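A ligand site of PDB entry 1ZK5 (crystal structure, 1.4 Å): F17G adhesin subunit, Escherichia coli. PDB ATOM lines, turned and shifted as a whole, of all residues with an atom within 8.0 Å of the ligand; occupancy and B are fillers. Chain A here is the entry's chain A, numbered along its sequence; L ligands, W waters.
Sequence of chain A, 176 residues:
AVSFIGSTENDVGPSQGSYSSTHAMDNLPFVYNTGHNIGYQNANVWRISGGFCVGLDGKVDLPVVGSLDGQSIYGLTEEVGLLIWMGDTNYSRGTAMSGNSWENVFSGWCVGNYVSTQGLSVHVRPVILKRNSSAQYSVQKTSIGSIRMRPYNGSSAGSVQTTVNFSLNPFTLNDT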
ATOM      1  N   ASN A  42     -18.960  29.632  12.948  1.00  0.00           N
ATOM      2  CA  ASN A  42     -17.848  28.995  13.611  1.00  0.00           C
ATOM      3  C   ASN A  42     -17.505  27.803  12.733  1.00  0.00           C
ATOM      4  O   ASN A  42     -18.333  26.916  12.526  1.00  0.00           O
ATOM      5  CB  ASN A  42     -18.247  28.494  14.994  1.00  0.00           C
ATOM      6  CG  ASN A  42     -17.053  28.059  15.816  1.00  0.00           C
ATOM      7  OD1 ASN A  42     -16.053  27.592  15.271  1.00  0.00           O
ATOM      8  ND2 ASN A  42     -17.139  28.205  17.132  1.00  0.00           N
ATOM      9  N   ALA A  43     -16.292  27.798  12.189  1.00  0.00           N
ATOM     10  CA  ALA A  43     -15.864  26.717  11.323  1.00  0.00           C
ATOM     11  C   ALA A  43     -15.525  25.444  12.084  1.00  0.00           C
ATOM     12  O   ALA A  43     -15.439  24.368  11.482  1.00  0.00           O
ATOM     13  CB  ALA A  43     -14.641  27.166  10.527  1.00  0.00           C
ATOM     14  N   ASN A  44     -15.357  25.547  13.399  1.00  0.00           N
ATOM     15  CA  ASN A  44     -14.945  24.388  14.190  1.00  0.00           C
ATOM     16  C   ASN A  44     -15.856  24.119  15.384  1.00  0.00           C
ATOM     17  O   ASN A  44     -15.523  24.484  16.518  1.00  0.00           O
ATOM     18  CB  ASN A  44     -13.515  24.625  14.648  1.00  0.00           C
ATOM     19  CG  ASN A  44     -12.608  25.045  13.498  1.00  0.00           C
ATOM     20  OD1 ASN A  44     -12.359  24.276  12.572  1.00  0.00           O
ATOM     21  ND2 ASN A  44     -12.129  26.288  13.554  1.00  0.00           N
ATOM     22  N   VAL A  45     -16.978  23.457  15.134  1.00  0.00           N
ATOM     23  CA  VAL A  45     -17.920  23.140  16.204  1.00  0.00           C
ATOM     24  C   VAL A  45     -17.783  21.680  16.660  1.00  0.00           C
ATOM     25  O   VAL A  45     -17.956  21.386  17.843  1.00  0.00           O
ATOM     26  CB  VAL A  45     -19.363  23.452  15.757  1.00  0.00           C
ATOM     27  CG1 VAL A  45     -20.338  23.106  16.865  1.00  0.00           C
ATOM     28  CG2 VAL A  45     -19.468  24.937  15.424  1.00  0.00           C
ATOM     29  N   TRP A  46     -17.498  20.783  15.722  1.00  0.00           N
ATOM     30  CA  TRP A  46     -17.279  19.379  16.054  1.00  0.00           C
ATOM     31  C   TRP A  46     -15.992  18.932  15.383  1.00  0.00           C
ATOM     32  O   TRP A  46     -15.687  19.351  14.266  1.00  0.00           O
ATOM     33  CB  TRP A  46     -18.408  18.490  15.520  1.00  0.00           C
ATOM     34  CG  TRP A  46     -19.706  18.658  16.205  1.00  0.00           C
ATOM     35  CD1 TRP A  46     -20.116  18.077  17.365  1.00  0.00           C
ATOM     36  CD2 TRP A  46     -20.769  19.507  15.781  1.00  0.00           C
ATOM     37  NE1 TRP A  46     -21.380  18.505  17.689  1.00  0.00           N
ATOM     38  CE2 TRP A  46     -21.801  19.395  16.733  1.00  0.00           C
ATOM     39  CE3 TRP A  46     -20.947  20.361  14.682  1.00  0.00           C
ATOM     40  CZ2 TRP A  46     -23.010  20.095  16.621  1.00  0.00           C
ATOM     41  CZ3 TRP A  46     -22.142  21.067  14.572  1.00  0.00           C
ATOM     42  CH2 TRP A  46     -23.153  20.933  15.536  1.00  0.00           C
ATOM     43  N   ILE A  48     -14.073  15.852  13.814  1.00  0.00           N
ATOM     44  CA  ILE A  48     -14.425  14.536  13.273  1.00  0.00           C
ATOM     45  C   ILE A  48     -13.224  13.856  12.650  1.00  0.00           C
ATOM     46  O   ILE A  48     -12.265  14.517  12.236  1.00  0.00           O
ATOM     47  CB  ILE A  48     -15.556  14.648  12.208  1.00  0.00           C
ATOM     48  CG1 ILE A  48     -15.114  15.545  11.052  1.00  0.00           C
ATOM     49  CG2 ILE A  48     -16.818  15.190  12.872  1.00  0.00           C
ATOM     50  CD1 ILE A  48     -16.130  15.601   9.921  1.00  0.00           C
ATOM     51  N   VAL A  54     -21.019  13.534   8.279  1.00  0.00           N
ATOM     52  CA  VAL A  54     -21.916  14.413   9.017  1.00  0.00           C
ATOM     53  C   VAL A  54     -22.461  15.572   8.189  1.00  0.00           C
ATOM     54  O   VAL A  54     -21.775  16.128   7.335  1.00  0.00           O
ATOM     55  CB  VAL A  54     -21.192  14.986  10.271  1.00  0.00           C
ATOM     56  CG1 VAL A  54     -20.062  15.924   9.850  1.00  0.00           C
ATOM     57  CG2 VAL A  54     -22.186  15.682  11.191  1.00  0.00           C
ATOM     58  N   LEU A  56     -25.852  18.800   8.634  1.00  0.00           N
ATOM     59  CA  LEU A  56     -26.453  19.650   9.653  1.00  0.00           C
ATOM     60  C   LEU A  56     -27.947  19.815   9.497  1.00  0.00           C
ATOM     61  O   LEU A  56     -28.456  19.925   8.375  1.00  0.00           O
ATOM     62  CB  LEU A  56     -25.859  21.070   9.609  1.00  0.00           C
ATOM     63  CG  LEU A  56     -24.381  21.328   9.852  1.00  0.00           C
ATOM     64  CD1 LEU A  56     -24.076  22.790   9.554  1.00  0.00           C
ATOM     65  CD2 LEU A  56     -23.997  20.977  11.289  1.00  0.00           C
ATOM     66  N   GLY A  87     -26.897  26.933   8.077  1.00  0.00           N
ATOM     67  CA  GLY A  87     -26.166  26.045   7.198  1.00  0.00           C
ATOM     68  C   GLY A  87     -24.744  25.812   7.637  1.00  0.00           C
ATOM     69  O   GLY A  87     -24.398  26.012   8.795  1.00  0.00           O
ATOM     70  N   ASP A  88     -23.931  25.387   6.668  1.00  0.00           N
ATOM     71  CA  ASP A  88     -22.529  25.100   6.874  1.00  0.00           C
ATOM     72  C   ASP A  88     -21.755  26.395   7.163  1.00  0.00           C
ATOM     73  O   ASP A  88     -22.298  27.493   7.058  1.00  0.00           O
ATOM     74  CB  ASP A  88     -22.004  24.381   5.626  1.00  0.00           C
ATOM     75  CG  ASP A  88     -20.637  23.753   5.821  1.00  0.00           C
ATOM     76  OD1 ASP A  88     -20.303  23.393   6.964  1.00  0.00           O
ATOM     77  OD2 ASP A  88     -19.914  23.597   4.813  1.00  0.00           O
ATOM     78  N   THR A  89     -20.488  26.238   7.522  1.00  0.00           N
ATOM     79  CA  THR A  89     -19.621  27.343   7.879  1.00  0.00           C
ATOM     80  C   THR A  89     -19.741  28.680   7.128  1.00  0.00           C
ATOM     81  O   THR A  89     -19.969  29.717   7.749  1.00  0.00           O
ATOM     82  CB  THR A  89     -18.171  26.863   7.813  1.00  0.00           C
ATOM     83  OG1 THR A  89     -18.024  25.752   8.716  1.00  0.00           O
ATOM     84  CG2 THR A  89     -17.197  27.973   8.207  1.00  0.00           C
ATOM     85  N   ASN A  90     -19.590  28.645   5.812  1.00  0.00           N
ATOM     86  CA  ASN A  90     -19.656  29.864   5.005  1.00  0.00           C
ATOM     87  C   ASN A  90     -21.058  30.453   4.936  1.00  0.00           C
ATOM     88  O   ASN A  90     -22.018  29.740   4.654  1.00  0.00           O
ATOM     89  CB  ASN A  90     -19.161  29.574   3.586  1.00  0.00           C
ATOM     90  CG  ASN A  90     -17.922  28.707   3.566  1.00  0.00           C
ATOM     91  OD1 ASN A  90     -16.972  28.944   4.298  1.00  0.00           O
ATOM     92  ND2 ASN A  90     -17.936  27.678   2.709  1.00  0.00           N
ATOM     93  N   ARG A  93     -23.421  29.796   1.940  1.00  0.00           N
ATOM     94  CA  ARG A  93     -24.046  28.506   1.714  1.00  0.00           C
ATOM     95  C   ARG A  93     -25.257  28.262   2.619  1.00  0.00           C
ATOM     96  O   ARG A  93     -25.728  27.141   2.750  1.00  0.00           O
ATOM     97  CB  ARG A  93     -23.006  27.398   1.898  1.00  0.00           C
ATOM     98  CG  ARG A  93     -21.931  27.430   0.822  1.00  0.00           C
ATOM     99  CD  ARG A  93     -20.954  26.287   0.999  1.00  0.00           C
ATOM    100  NE  ARG A  93     -20.098  26.132  -0.172  1.00  0.00           N
ATOM    101  CZ  ARG A  93     -20.552  25.840  -1.392  1.00  0.00           C
ATOM    102  NH1 ARG A  93     -19.701  25.712  -2.404  1.00  0.00           N
ATOM    103  NH2 ARG A  93     -21.846  25.666  -1.603  1.00  0.00           N
ATOM    104  N   PHE A 106     -27.507  21.441   5.592  1.00  0.00           N
ATOM    105  CA  PHE A 106     -26.213  21.127   4.996  1.00  0.00           C
ATOM    106  C   PHE A 106     -26.244  19.637   4.689  1.00  0.00           C
ATOM    107  O   PHE A 106     -26.300  18.812   5.600  1.00  0.00           O
ATOM    108  CB  PHE A 106     -25.037  21.449   5.931  1.00  0.00           C
ATOM    109  CG  PHE A 106     -23.706  20.938   5.430  1.00  0.00           C
ATOM    110  CD1 PHE A 106     -23.305  21.151   4.113  1.00  0.00           C
ATOM    111  CD2 PHE A 106     -22.850  20.236   6.279  1.00  0.00           C
ATOM    112  CE1 PHE A 106     -22.089  20.670   3.639  1.00  0.00           C
ATOM    113  CE2 PHE A 106     -21.635  19.750   5.822  1.00  0.00           C
ATOM    114  CZ  PHE A 106     -21.250  19.967   4.499  1.00  0.00           C
ATOM    115  N   GLY A 108     -24.108  17.565   3.902  1.00  0.00           N
ATOM    116  CA  GLY A 108     -23.081  16.781   4.548  1.00  0.00           C
ATOM    117  C   GLY A 108     -21.865  16.352   3.752  1.00  0.00           C
ATOM    118  O   GLY A 108     -21.820  16.475   2.526  1.00  0.00           O
ATOM    119  N   TRP A 109     -20.864  15.861   4.477  1.00  0.00           N
ATOM    120  CA  TRP A 109     -19.637  15.370   3.857  1.00  0.00           C
ATOM    121  C   TRP A 109     -19.059  14.305   4.779  1.00  0.00           C
ATOM    122  O   TRP A 109     -19.492  14.148   5.925  1.00  0.00           O
ATOM    123  CB  TRP A 109     -18.619  16.485   3.663  1.00  0.00           C
ATOM    124  CG  TRP A 109     -17.950  16.962   4.917  1.00  0.00           C
ATOM    125  CD1 TRP A 109     -18.545  17.556   5.993  1.00  0.00           C
ATOM    126  CD2 TRP A 109     -16.549  16.901   5.214  1.00  0.00           C
ATOM    127  NE1 TRP A 109     -17.603  17.886   6.939  1.00  0.00           N
ATOM    128  CE2 TRP A 109     -16.366  17.499   6.488  1.00  0.00           C
ATOM    129  CE3 TRP A 109     -15.431  16.425   4.520  1.00  0.00           C
ATOM    130  CZ2 TRP A 109     -15.102  17.613   7.083  1.00  0.00           C
ATOM    131  CZ3 TRP A 109     -14.176  16.539   5.121  1.00  0.00           C
ATOM    132  CH2 TRP A 109     -14.026  17.131   6.380  1.00  0.00           C
ATOM    133  N   CYS A 110     -18.081  13.563   4.267  1.00  0.00           N
ATOM    134  CA  CYS A 110     -17.431  12.514   5.029  1.00  0.00           C
ATOM    135  C   CYS A 110     -15.934  12.781   5.083  1.00  0.00           C
ATOM    136  O   CYS A 110     -15.301  12.953   4.041  1.00  0.00           O
ATOM    137  CB  CYS A 110     -17.639  11.158   4.356  1.00  0.00           C
ATOM    138  SG  CYS A 110     -19.371  10.650   4.197  1.00  0.00           S
ATOM    139  N   TYR A 114      -8.369  10.882   8.597  1.00  0.00           N
ATOM    140  CA  TYR A 114      -7.589  11.960   9.184  1.00  0.00           C
ATOM    141  C   TYR A 114      -8.565  12.780  10.032  1.00  0.00           C
ATOM    142  O   TYR A 114      -9.752  12.456  10.096  1.00  0.00           O
ATOM    143  CB  TYR A 114      -6.946  12.855   8.114  1.00  0.00           C
ATOM    144  CG  TYR A 114      -7.915  13.452   7.120  1.00  0.00           C
ATOM    145  CD1 TYR A 114      -8.383  12.703   6.036  1.00  0.00           C
ATOM    146  CD2 TYR A 114      -8.401  14.752   7.283  1.00  0.00           C
ATOM    147  CE1 TYR A 114      -9.304  13.232   5.146  1.00  0.00           C
ATOM    148  CE2 TYR A 114      -9.325  15.290   6.388  1.00  0.00           C
ATOM    149  CZ  TYR A 114      -9.767  14.524   5.324  1.00  0.00           C
ATOM    150  OH  TYR A 114     -10.702  15.044   4.448  1.00  0.00           O
ATOM    151  N   VAL A 115      -8.057  13.831  10.659  1.00  0.00           N
ATOM    152  CA  VAL A 115      -8.866  14.667  11.526  1.00  0.00           C
ATOM    153  C   VAL A 115      -9.246  15.999  10.889  1.00  0.00           C
ATOM    154  O   VAL A 115      -8.430  16.663  10.259  1.00  0.00           O
ATOM    155  CB  VAL A 115      -8.120  14.980  12.843  1.00  0.00           C
ATOM    156  CG1 VAL A 115      -8.994  15.825  13.758  1.00  0.00           C
ATOM    157  CG2 VAL A 115      -7.707  13.680  13.533  1.00  0.00           C
ATOM    158  N   SER A 116     -10.507  16.386  11.050  1.00  0.00           N
ATOM    159  CA  SER A 116     -10.980  17.653  10.522  1.00  0.00           C
ATOM    160  C   SER A 116     -12.093  18.175  11.410  1.00  0.00           C
ATOM    161  O   SER A 116     -12.263  17.716  12.545  1.00  0.00           O
ATOM    162  CB  SER A 116     -11.462  17.508   9.073  1.00  0.00           C
ATOM    163  OG  SER A 116     -11.696  18.773   8.489  1.00  0.00           O
ATOM    164  N   THR A 117     -12.864  19.132  10.911  1.00  0.00           N
ATOM    165  CA  THR A 117     -13.949  19.702  11.699  1.00  0.00           C
ATOM    166  C   THR A 117     -15.198  19.978  10.888  1.00  0.00           C
ATOM    167  O   THR A 117     -15.164  19.993   9.653  1.00  0.00           O
ATOM    168  CB  THR A 117     -13.541  21.039  12.364  1.00  0.00           C
ATOM    169  OG1 THR A 117     -13.243  21.998  11.339  1.00  0.00           O
ATOM    170  CG2 THR A 117     -12.319  20.864  13.251  1.00  0.00           C
ATOM    171  N   GLN A 118     -16.300  20.163  11.599  1.00  0.00           N
ATOM    172  CA  GLN A 118     -17.586  20.504  11.010  1.00  0.00           C
ATOM    173  C   GLN A 118     -17.993  21.819  11.656  1.00  0.00           C
ATOM    174  O   GLN A 118     -17.962  21.949  12.895  1.00  0.00           O
ATOM    175  CB  GLN A 118     -18.628  19.430  11.299  1.00  0.00           C
ATOM    176  CG  GLN A 118     -20.047  19.763  10.799  1.00  0.00           C
ATOM    177  CD  GLN A 118     -20.084  20.086   9.320  1.00  0.00           C
ATOM    178  OE1 GLN A 118     -19.542  19.349   8.495  1.00  0.00           O
ATOM    179  NE2 GLN A 118     -20.745  21.192   8.966  1.00  0.00           N
ATOM    180  N   GLY A 119     -18.358  22.789  10.829  1.00  0.00           N
ATOM    181  CA  GLY A 119     -18.755  24.089  11.345  1.00  0.00           C
ATOM    182  C   GLY A 119     -20.193  24.409  10.996  1.00  0.00           C
ATOM    183  O   GLY A 119     -20.945  23.534  10.561  1.00  0.00           O
ATOM    184  N   LEU A 120     -20.577  25.673  11.182  1.00  0.00           N
ATOM    185  CA  LEU A 120     -21.932  26.089  10.896  1.00  0.00           C
ATOM    186  C   LEU A 120     -22.007  27.613  10.865  1.00  0.00           C
ATOM    187  O   LEU A 120     -21.059  28.301  11.236  1.00  0.00           O
ATOM    188  CB  LEU A 120     -22.868  25.548  11.991  1.00  0.00           C
ATOM    189  CG  LEU A 120     -22.586  25.948  13.452  1.00  0.00           C
ATOM    190  CD1 LEU A 120     -22.976  27.403  13.700  1.00  0.00           C
ATOM    191  CD2 LEU A 120     -23.382  25.050  14.382  1.00  0.00           C
ATOM    192  N   SER A 121     -23.133  28.128  10.389  1.00  0.00           N
ATOM    193  CA  SER A 121     -23.344  29.566  10.363  1.00  0.00           C
ATOM    194  C   SER A 121     -24.828  29.835  10.377  1.00  0.00           C
ATOM    195  O   SER A 121     -25.634  28.989   9.972  1.00  0.00           O
ATOM    196  CB  SER A 121     -22.723  30.213   9.111  1.00  0.00           C
ATOM    197  OG  SER A 121     -23.452  29.898   7.944  1.00  0.00           O
HETATM  198  C1  LIG L   1     -14.325  21.688   6.647  1.00  0.00           C
HETATM  199  C2  LIG L   1     -14.530  23.120   7.083  1.00  0.00           C
HETATM  200  C3  LIG L   1     -15.646  22.998   8.107  1.00  0.00           C
HETATM  201  C4  LIG L   1     -16.894  22.664   7.315  1.00  0.00           C
HETATM  202  C5  LIG L   1     -16.678  21.339   6.543  1.00  0.00           C
HETATM  203  C6  LIG L   1     -17.777  21.066   5.529  1.00  0.00           C
HETATM  204  C7  LIG L   1     -12.094  23.551   8.263  1.00  0.00           C
HETATM  205  C8  LIG L   1     -10.998  23.712   9.280  1.00  0.00           C
HETATM  206  N1  LIG L   1     -13.409  22.873   8.355  1.00  0.00           N
HETATM  207  O1  LIG L   1     -13.165  21.564   5.903  1.00  0.00           O
HETATM  208  O2  LIG L   1     -15.794  24.197   8.844  1.00  0.00           O
HETATM  209  O3  LIG L   1     -18.025  22.554   8.155  1.00  0.00           O
HETATM  210  O4  LIG L   1     -15.426  21.344   5.823  1.00  0.00           O
HETATM  211  O5  LIG L   1     -17.842  22.110   4.563  1.00  0.00           O
HETATM  212  O6  LIG L   1     -12.010  24.161   7.211  1.00  0.00           O
HETATM  213  O   HOH W   1     -17.860  20.703   2.413  1.00  0.00           O
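The side-chain amide nitrogen (NE2) of Gln 118 sits at hydrogen-bond distance from the side-chain carboxylate (OD1) of Asp 88 (3.0 Å). The backbone carbonyl oxygen (O) of Ala 43 lies close to the backbone NH (N) of Gly 119, 3.4 Å away. The backbone carbonyl oxygen of Ala 43 is in hydrogen-bond range of the side-chain hydroxyl of Thr 117, at 3.2 Å. O of Thr 89 sits close to OG of Ser 121 (3.5 Å). The side-chain hydroxyl of Thr 117 sits at hydrogen-bond distance from the side-chain amide oxygen of Asn 44 (2.7 Å). The backbone NH (N) of Gln 118 sits at hydrogen-bond distance from the backbone carbonyl oxygen (O) of Trp 46 (2.9 Å). The backbone carbonyl oxygen of Trp 109 lies within hydrogen-bond range of the backbone NH of Val 54, at 2.9 Å. N of Asn 44 sits at hydrogen-bond distance from OD1 of Asn 42, 2.9 Å away.
Residues that only touch the ligand: Trp 109, Asn 44 and Phe 106. Hydrophobic or aromatic side chains that line the ligand: Ala 43, Phe 106 and Trp 109. Along chain A the residues within 4 Å of the ligand span positions 43 to 119.
O5 of the ligand is in hydrogen-bond range of OD2 of Asp 88, 2.6 Å away. An oxygen (O2) of the ligand is in hydrogen-bond range of the backbone carbonyl oxygen (O) of Ala 43 (2.7 Å). The backbone NH of Gly 119 lies within hydrogen-bond range of an oxygen (O3) of the ligand, 2.7 Å away. OG1 of Thr 89 is in hydrogen-bond range of O2 of the ligand (2.7 Å). A nitrogen (N1) of the ligand sits at hydrogen-bond distance from the side-chain hydroxyl (OG1) of Thr 117. An oxygen (O3) of the ligand lies within hydrogen-bond range of the side-chain amide nitrogen (NE2) of Gln 118 (3.1 Å).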
